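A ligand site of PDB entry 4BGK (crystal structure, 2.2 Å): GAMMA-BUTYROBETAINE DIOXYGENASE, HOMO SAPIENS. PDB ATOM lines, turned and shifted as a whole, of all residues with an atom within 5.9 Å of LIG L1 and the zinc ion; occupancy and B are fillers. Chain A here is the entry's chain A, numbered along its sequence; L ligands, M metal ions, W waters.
OD2 of Asp 204 lies close to OE1 of Gln 215, 3.3 Å away. OD2 of Asp 204 sits at hydrogen-bond distance from OH of Tyr 366, at 2.5 Å. The guanidinium group (NH2) of Arg 360 sits at hydrogen-bond distance from the backbone carbonyl oxygen (O) of Gly 227, 2.9 Å away. O of Ala 193 is in hydrogen-bond range of NH1 of Arg 349. O of Arg 349 lies within hydrogen-bond range of N of Leu 199, at 2.9 Å. The side-chain amide oxygen (OD1) of Asn 191 lies within hydrogen-bond range of the backbone NH (N) of Ala 193, 3.0 Å away. The backbone carbonyl oxygen (O) of Leu 362 is in hydrogen-bond range of the backbone NH (N) of Val 183 (2.7 Å).
Residues that only touch LIG L1: Val 183, Ala 193, Leu 199, Leu 217 and Leu 362. Hydrophobic or aromatic side chains within 4 Å of LIG L1: Val 183, Ala 193, Leu 199, His 202, Leu 217, His 347 and Leu 362. Of the 22 residues printed, 10 come within 4 Å of LIG L1.
The guanidinium group (NH2) of Arg 360 is in salt-bridge range of an oxygen (O4) of LIG L1 (2.9 Å). NH1 of Arg 349 lies within salt-bridge range of O5 of LIG L1, 3.0 Å away. The side-chain amide nitrogen (ND2) of Asn 191 sits at hydrogen-bond distance from an oxygen (O2) of LG2 L2 (2.9 Å). The side-chain amide nitrogen of Asn 292 sits at hydrogen-bond distance from an oxygen (O1) of LG2 L2, at 2.8 Å.
Water W1 lies within hydrogen-bond range of O4 of LIG L1, OG of Ser 229 and O of Gly 348.
Three residues have an atom within 4 Å of the zinc ion: His 202, Asp 204 and His 347. The nearest printed residue that does not touch the zinc ion is Gln 215 (4.03 Å).
The zinc ion is bound by O2 of LIG L1 (1.9 Å). The zinc ion is bound by OD1 of Asp 204, at 2.1 Å. The zinc ion is bound by a ring nitrogen (NE2) of His 202 (2.2 Å). The zinc ion is bound by NE2 of His 347 (2.2 Å). The zinc ion is bound by an oxygen (O3) of LIG L1. The zinc ion has five donor atoms within binding distance.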
ATOM      1  N   TRP A 181      29.382  14.645   9.573  1.00  0.00           N
ATOM      2  CA  TRP A 181      29.048  14.577  11.006  1.00  0.00           C
ATOM      3  C   TRP A 181      27.574  14.295  11.186  1.00  0.00           C
ATOM      4  O   TRP A 181      26.753  14.571  10.293  1.00  0.00           O
ATOM      5  CB  TRP A 181      29.432  15.850  11.755  1.00  0.00           C
ATOM      6  CG  TRP A 181      29.509  17.073  10.906  1.00  0.00           C
ATOM      7  CD1 TRP A 181      30.591  17.543  10.270  1.00  0.00           C
ATOM      8  CD2 TRP A 181      28.440  17.981  10.595  1.00  0.00           C
ATOM      9  NE1 TRP A 181      30.278  18.673   9.564  1.00  0.00           N
ATOM     10  CE2 TRP A 181      28.958  18.974   9.749  1.00  0.00           C
ATOM     11  CE3 TRP A 181      27.086  18.042  10.953  1.00  0.00           C
ATOM     12  CZ2 TRP A 181      28.199  20.004   9.254  1.00  0.00           C
ATOM     13  CZ3 TRP A 181      26.341  19.068  10.461  1.00  0.00           C
ATOM     14  CH2 TRP A 181      26.887  20.038   9.623  1.00  0.00           C
ATOM     15  N   VAL A 183      24.116  14.792  13.090  1.00  0.00           N
ATOM     16  CA  VAL A 183      23.319  15.639  13.966  1.00  0.00           C
ATOM     17  C   VAL A 183      22.260  14.759  14.606  1.00  0.00           C
ATOM     18  O   VAL A 183      21.299  14.343  13.961  1.00  0.00           O
ATOM     19  CB  VAL A 183      22.645  16.804  13.220  1.00  0.00           C
ATOM     20  CG1 VAL A 183      21.953  17.726  14.212  1.00  0.00           C
ATOM     21  CG2 VAL A 183      23.677  17.537  12.382  1.00  0.00           C
ATOM     22  N   ASN A 191      28.500  19.623  21.617  1.00  0.00           N
ATOM     23  CA  ASN A 191      27.949  20.740  20.834  1.00  0.00           C
ATOM     24  C   ASN A 191      26.458  20.773  21.047  1.00  0.00           C
ATOM     25  O   ASN A 191      25.833  19.722  21.125  1.00  0.00           O
ATOM     26  CB  ASN A 191      28.287  20.561  19.357  1.00  0.00           C
ATOM     27  CG  ASN A 191      28.060  21.827  18.536  1.00  0.00           C
ATOM     28  OD1 ASN A 191      26.942  22.135  18.135  1.00  0.00           O
ATOM     29  ND2 ASN A 191      29.146  22.533  18.231  1.00  0.00           N
ATOM     30  N   ALA A 193      24.205  21.439  19.095  1.00  0.00           N
ATOM     31  CA  ALA A 193      23.533  20.827  17.954  1.00  0.00           C
ATOM     32  C   ALA A 193      23.228  19.361  18.202  1.00  0.00           C
ATOM     33  O   ALA A 193      22.250  18.816  17.678  1.00  0.00           O
ATOM     34  CB  ALA A 193      24.374  20.983  16.701  1.00  0.00           C
ATOM     35  N   TYR A 194      24.050  18.716  19.019  1.00  0.00           N
ATOM     36  CA  TYR A 194      23.908  17.280  19.264  1.00  0.00           C
ATOM     37  C   TYR A 194      23.120  17.039  20.561  1.00  0.00           C
ATOM     38  O   TYR A 194      23.477  16.173  21.365  1.00  0.00           O
ATOM     39  CB  TYR A 194      25.283  16.609  19.338  1.00  0.00           C
ATOM     40  CG  TYR A 194      26.196  16.799  18.123  1.00  0.00           C
ATOM     41  CD1 TYR A 194      25.679  16.963  16.826  1.00  0.00           C
ATOM     42  CD2 TYR A 194      27.574  16.760  18.269  1.00  0.00           C
ATOM     43  CE1 TYR A 194      26.511  17.107  15.732  1.00  0.00           C
ATOM     44  CE2 TYR A 194      28.430  16.908  17.179  1.00  0.00           C
ATOM     45  CZ  TYR A 194      27.886  17.089  15.923  1.00  0.00           C
ATOM     46  OH  TYR A 194      28.730  17.239  14.854  1.00  0.00           O
ATOM     47  N   LEU A 199      17.718  25.368  18.275  1.00  0.00           N
ATOM     48  CA  LEU A 199      18.800  26.177  17.802  1.00  0.00           C
ATOM     49  C   LEU A 199      18.156  27.404  17.219  1.00  0.00           C
ATOM     50  O   LEU A 199      17.352  27.312  16.282  1.00  0.00           O
ATOM     51  CB  LEU A 199      19.599  25.429  16.724  1.00  0.00           C
ATOM     52  CG  LEU A 199      20.197  24.121  17.221  1.00  0.00           C
ATOM     53  CD1 LEU A 199      20.897  23.403  16.086  1.00  0.00           C
ATOM     54  CD2 LEU A 199      21.152  24.369  18.360  1.00  0.00           C
ATOM     55  N   HIS A 202      21.492  31.037  13.531  1.00  0.00           N
ATOM     56  CA  HIS A 202      22.930  31.135  13.646  1.00  0.00           C
ATOM     57  C   HIS A 202      23.537  30.770  12.330  1.00  0.00           C
ATOM     58  O   HIS A 202      22.901  30.107  11.498  1.00  0.00           O
ATOM     59  CB  HIS A 202      23.438  30.154  14.729  1.00  0.00           C
ATOM     60  CG  HIS A 202      23.266  28.708  14.372  1.00  0.00           C
ATOM     61  ND1 HIS A 202      22.069  28.044  14.485  1.00  0.00           N
ATOM     62  CD2 HIS A 202      24.146  27.804  13.896  1.00  0.00           C
ATOM     63  CE1 HIS A 202      22.216  26.797  14.089  1.00  0.00           C
ATOM     64  NE2 HIS A 202      23.471  26.624  13.734  1.00  0.00           N
ATOM     65  N   THR A 203      24.773  31.194  12.130  1.00  0.00           N
ATOM     66  CA  THR A 203      25.654  30.625  11.121  1.00  0.00           C
ATOM     67  C   THR A 203      26.498  29.572  11.782  1.00  0.00           C
ATOM     68  O   THR A 203      26.712  29.628  12.990  1.00  0.00           O
ATOM     69  CB  THR A 203      26.578  31.690  10.474  1.00  0.00           C
ATOM     70  OG1 THR A 203      27.494  32.264  11.421  1.00  0.00           O
ATOM     71  CG2 THR A 203      25.746  32.802   9.848  1.00  0.00           C
ATOM     72  N   ASP A 204      27.004  28.620  10.998  1.00  0.00           N
ATOM     73  CA  ASP A 204      27.889  27.574  11.518  1.00  0.00           C
ATOM     74  C   ASP A 204      29.360  28.006  11.542  1.00  0.00           C
ATOM     75  O   ASP A 204      29.836  28.656  10.609  1.00  0.00           O
ATOM     76  CB  ASP A 204      27.759  26.262  10.731  1.00  0.00           C
ATOM     77  CG  ASP A 204      26.722  25.330  11.334  1.00  0.00           C
ATOM     78  OD1 ASP A 204      25.775  25.844  11.907  1.00  0.00           O
ATOM     79  OD2 ASP A 204      26.859  24.093  11.236  1.00  0.00           O
ATOM     80  N   GLN A 215      26.927  24.752   3.439  1.00  0.00           N
ATOM     81  CA  GLN A 215      26.635  23.691   4.364  1.00  0.00           C
ATOM     82  C   GLN A 215      25.648  22.740   3.690  1.00  0.00           C
ATOM     83  O   GLN A 215      24.759  23.165   2.984  1.00  0.00           O
ATOM     84  CB  GLN A 215      26.030  24.282   5.639  1.00  0.00           C
ATOM     85  CG  GLN A 215      25.579  23.246   6.634  1.00  0.00           C
ATOM     86  CD  GLN A 215      25.327  23.825   8.009  1.00  0.00           C
ATOM     87  OE1 GLN A 215      24.741  23.154   8.855  1.00  0.00           O
ATOM     88  NE2 GLN A 215      25.756  25.064   8.232  1.00  0.00           N
ATOM     89  N   LEU A 217      22.969  19.501   4.541  1.00  0.00           N
ATOM     90  CA  LEU A 217      22.268  18.733   5.586  1.00  0.00           C
ATOM     91  C   LEU A 217      21.279  17.747   4.969  1.00  0.00           C
ATOM     92  O   LEU A 217      20.354  18.108   4.223  1.00  0.00           O
ATOM     93  CB  LEU A 217      21.514  19.652   6.543  1.00  0.00           C
ATOM     94  CG  LEU A 217      22.309  20.419   7.603  1.00  0.00           C
ATOM     95  CD1 LEU A 217      21.368  21.314   8.405  1.00  0.00           C
ATOM     96  CD2 LEU A 217      23.029  19.475   8.535  1.00  0.00           C
ATOM     97  N   GLY A 227      11.524  19.723  15.567  1.00  0.00           N
ATOM     98  CA  GLY A 227      12.658  19.567  14.655  1.00  0.00           C
ATOM     99  C   GLY A 227      12.475  20.192  13.293  1.00  0.00           C
ATOM    100  O   GLY A 227      13.241  19.886  12.377  1.00  0.00           O
ATOM    101  N   ASP A 228      11.500  21.097  13.172  1.00  0.00           N
ATOM    102  CA  ASP A 228      11.312  21.949  12.004  1.00  0.00           C
ATOM    103  C   ASP A 228      12.542  22.807  11.794  1.00  0.00           C
ATOM    104  O   ASP A 228      13.206  23.165  12.730  1.00  0.00           O
ATOM    105  CB  ASP A 228      10.098  22.879  12.173  1.00  0.00           C
ATOM    106  CG  ASP A 228       8.841  22.124  12.554  1.00  0.00           C
ATOM    107  OD1 ASP A 228       8.738  21.676  13.718  1.00  0.00           O
ATOM    108  OD2 ASP A 228       7.979  21.975  11.691  1.00  0.00           O
ATOM    109  N   SER A 229      12.795  23.146  10.547  1.00  0.00           N
ATOM    110  CA  SER A 229      13.892  24.005  10.183  1.00  0.00           C
ATOM    111  C   SER A 229      13.372  25.396   9.973  1.00  0.00           C
ATOM    112  O   SER A 229      12.203  25.621   9.610  1.00  0.00           O
ATOM    113  CB  SER A 229      14.544  23.514   8.886  1.00  0.00           C
ATOM    114  OG  SER A 229      14.918  22.147   8.965  1.00  0.00           O
ATOM    115  N   ASN A 292      26.974  32.788  15.967  1.00  0.00           N
ATOM    116  CA  ASN A 292      26.367  31.672  16.654  1.00  0.00           C
ATOM    117  C   ASN A 292      26.362  31.975  18.151  1.00  0.00           C
ATOM    118  O   ASN A 292      27.419  32.136  18.776  1.00  0.00           O
ATOM    119  CB  ASN A 292      27.086  30.374  16.314  1.00  0.00           C
ATOM    120  CG  ASN A 292      26.408  29.152  16.925  1.00  0.00           C
ATOM    121  OD1 ASN A 292      25.570  29.284  17.839  1.00  0.00           O
ATOM    122  ND2 ASN A 292      26.782  27.965  16.454  1.00  0.00           N
ATOM    123  N   MET A 332      12.124  19.026   7.155  1.00  0.00           N
ATOM    124  CA  MET A 332      12.832  18.075   6.324  1.00  0.00           C
ATOM    125  C   MET A 332      12.260  16.667   6.523  1.00  0.00           C
ATOM    126  O   MET A 332      11.924  16.314   7.644  1.00  0.00           O
ATOM    127  CB  MET A 332      14.313  18.087   6.665  1.00  0.00           C
ATOM    128  CG  MET A 332      15.031  19.348   6.210  1.00  0.00           C
ATOM    129  SD  MET A 332      16.813  19.237   6.521  1.00  0.00           S
ATOM    130  CE  MET A 332      17.282  18.233   5.110  1.00  0.00           C
ATOM    131  N   HIS A 347      20.357  29.888  10.082  1.00  0.00           N
ATOM    132  CA  HIS A 347      19.471  28.759  10.158  1.00  0.00           C
ATOM    133  C   HIS A 347      19.278  28.298  11.567  1.00  0.00           C
ATOM    134  O   HIS A 347      20.056  28.633  12.503  1.00  0.00           O
ATOM    135  CB  HIS A 347      20.000  27.638   9.293  1.00  0.00           C
ATOM    136  CG  HIS A 347      21.295  27.072   9.748  1.00  0.00           C
ATOM    137  ND1 HIS A 347      22.492  27.759   9.637  1.00  0.00           N
ATOM    138  CD2 HIS A 347      21.593  25.874  10.318  1.00  0.00           C
ATOM    139  CE1 HIS A 347      23.464  27.000  10.123  1.00  0.00           C
ATOM    140  NE2 HIS A 347      22.942  25.872  10.549  1.00  0.00           N
ATOM    141  N   GLY A 348      18.193  27.566  11.758  1.00  0.00           N
ATOM    142  CA  GLY A 348      17.882  27.053  13.076  1.00  0.00           C
ATOM    143  C   GLY A 348      16.957  25.869  13.040  1.00  0.00           C
ATOM    144  O   GLY A 348      16.566  25.373  11.970  1.00  0.00           O
ATOM    145  N   ARG A 349      16.552  25.461  14.215  1.00  0.00           N
ATOM    146  CA  ARG A 349      15.777  24.255  14.363  1.00  0.00           C
ATOM    147  C   ARG A 349      14.913  24.359  15.625  1.00  0.00           C
ATOM    148  O   ARG A 349      15.375  24.829  16.676  1.00  0.00           O
ATOM    149  CB  ARG A 349      16.721  23.058  14.428  1.00  0.00           C
ATOM    150  CG  ARG A 349      16.221  21.916  15.280  1.00  0.00           C
ATOM    151  CD  ARG A 349      17.272  20.863  15.523  1.00  0.00           C
ATOM    152  NE  ARG A 349      17.832  20.902  16.860  1.00  0.00           N
ATOM    153  CZ  ARG A 349      19.032  20.422  17.186  1.00  0.00           C
ATOM    154  NH1 ARG A 349      19.819  19.879  16.262  1.00  0.00           N
ATOM    155  NH2 ARG A 349      19.445  20.516  18.442  1.00  0.00           N
ATOM    156  N   ARG A 360      15.755  11.173  15.430  1.00  0.00           N
ATOM    157  CA  ARG A 360      16.100  12.247  14.524  1.00  0.00           C
ATOM    158  C   ARG A 360      17.594  12.219  14.205  1.00  0.00           C
ATOM    159  O   ARG A 360      18.421  12.180  15.116  1.00  0.00           O
ATOM    160  CB  ARG A 360      15.744  13.610  15.111  1.00  0.00           C
ATOM    161  CG  ARG A 360      15.779  14.713  14.063  1.00  0.00           C
ATOM    162  CD  ARG A 360      15.441  16.044  14.657  1.00  0.00           C
ATOM    163  NE  ARG A 360      15.298  17.109  13.670  1.00  0.00           N
ATOM    164  CZ  ARG A 360      16.250  17.951  13.282  1.00  0.00           C
ATOM    165  NH1 ARG A 360      17.517  17.846  13.730  1.00  0.00           N
ATOM    166  NH2 ARG A 360      15.963  18.883  12.405  1.00  0.00           N
ATOM    167  N   LEU A 362      20.389  13.805  11.230  1.00  0.00           N
ATOM    168  CA  LEU A 362      20.869  14.400   9.997  1.00  0.00           C
ATOM    169  C   LEU A 362      22.355  14.092   9.807  1.00  0.00           C
ATOM    170  O   LEU A 362      23.076  13.870  10.782  1.00  0.00           O
ATOM    171  CB  LEU A 362      20.614  15.894   9.981  1.00  0.00           C
ATOM    172  CG  LEU A 362      19.315  16.467  10.513  1.00  0.00           C
ATOM    173  CD1 LEU A 362      19.380  17.991  10.403  1.00  0.00           C
ATOM    174  CD2 LEU A 362      18.081  15.937   9.793  1.00  0.00           C
ATOM    175  N   TYR A 366      30.451  20.379   5.109  1.00  0.00           N
ATOM    176  CA  TYR A 366      30.703  21.727   4.683  1.00  0.00           C
ATOM    177  C   TYR A 366      31.453  21.713   3.347  1.00  0.00           C
ATOM    178  O   TYR A 366      32.163  20.754   3.038  1.00  0.00           O
ATOM    179  CB  TYR A 366      31.559  22.435   5.720  1.00  0.00           C
ATOM    180  CG  TYR A 366      30.905  22.616   7.081  1.00  0.00           C
ATOM    181  CD1 TYR A 366      29.682  23.304   7.204  1.00  0.00           C
ATOM    182  CD2 TYR A 366      31.493  22.105   8.223  1.00  0.00           C
ATOM    183  CE1 TYR A 366      29.092  23.485   8.446  1.00  0.00           C
ATOM    184  CE2 TYR A 366      30.909  22.269   9.451  1.00  0.00           C
ATOM    185  CZ  TYR A 366      29.725  22.978   9.566  1.00  0.00           C
ATOM    186  OH  TYR A 366      29.160  23.119  10.806  1.00  0.00           O
HETATM  187  C1  LIG L   1      23.642  22.364  13.018  1.00  0.00           C
HETATM  188  C2  LIG L   1      22.243  22.696  12.688  1.00  0.00           C
HETATM  189  C3  LIG L   1      19.993  22.002  12.079  1.00  0.00           C
HETATM  190  C4  LIG L   1      19.040  20.902  12.500  1.00  0.00           C
HETATM  191  O1  LIG L   1      23.947  21.175  13.334  1.00  0.00           O
HETATM  192  O2  LIG L   1      24.503  23.287  12.958  1.00  0.00           O
HETATM  193  O3  LIG L   1      21.958  23.854  12.474  1.00  0.00           O
HETATM  194  O4  LIG L   1      17.902  20.951  12.005  1.00  0.00           O
HETATM  195  N1  LIG L   1      21.337  21.730  12.580  1.00  0.00           N
HETATM  196  O5  LIG L   1      19.400  20.019  13.330  1.00  0.00           O
HETATM  197  O1  LG2 L   2      29.034  26.921  15.079  1.00  0.00           O
HETATM  198  P1  LG2 L   2      28.857  25.451  15.292  1.00  0.00           P
HETATM  199  O2  LG2 L   2      29.292  25.010  16.681  1.00  0.00           O
HETATM  200  C1  LG2 L   2      29.763  24.589  13.976  1.00  0.00           C
HETATM  201  C2  LG2 L   2      29.771  23.081  14.192  1.00  0.00           C
HETATM  202  C3  LG2 L   2      28.383  22.508  13.964  1.00  0.00           C
HETATM  203  N1  LG2 L   2      28.299  21.022  13.977  1.00  0.00           N
HETATM  204  C4  LG2 L   2      28.626  20.440  15.300  1.00  0.00           C
HETATM  205  C5  LG2 L   2      29.153  20.401  12.945  1.00  0.00           C
HETATM  206  C6  LG2 L   2      26.881  20.723  13.678  1.00  0.00           C
HETATM  207 ZN    ZN M   1      23.870  25.017  12.323  1.00  0.00          ZN
HETATM  208  O   HOH W   1      17.267  22.870  10.435  1.00  0.00           O
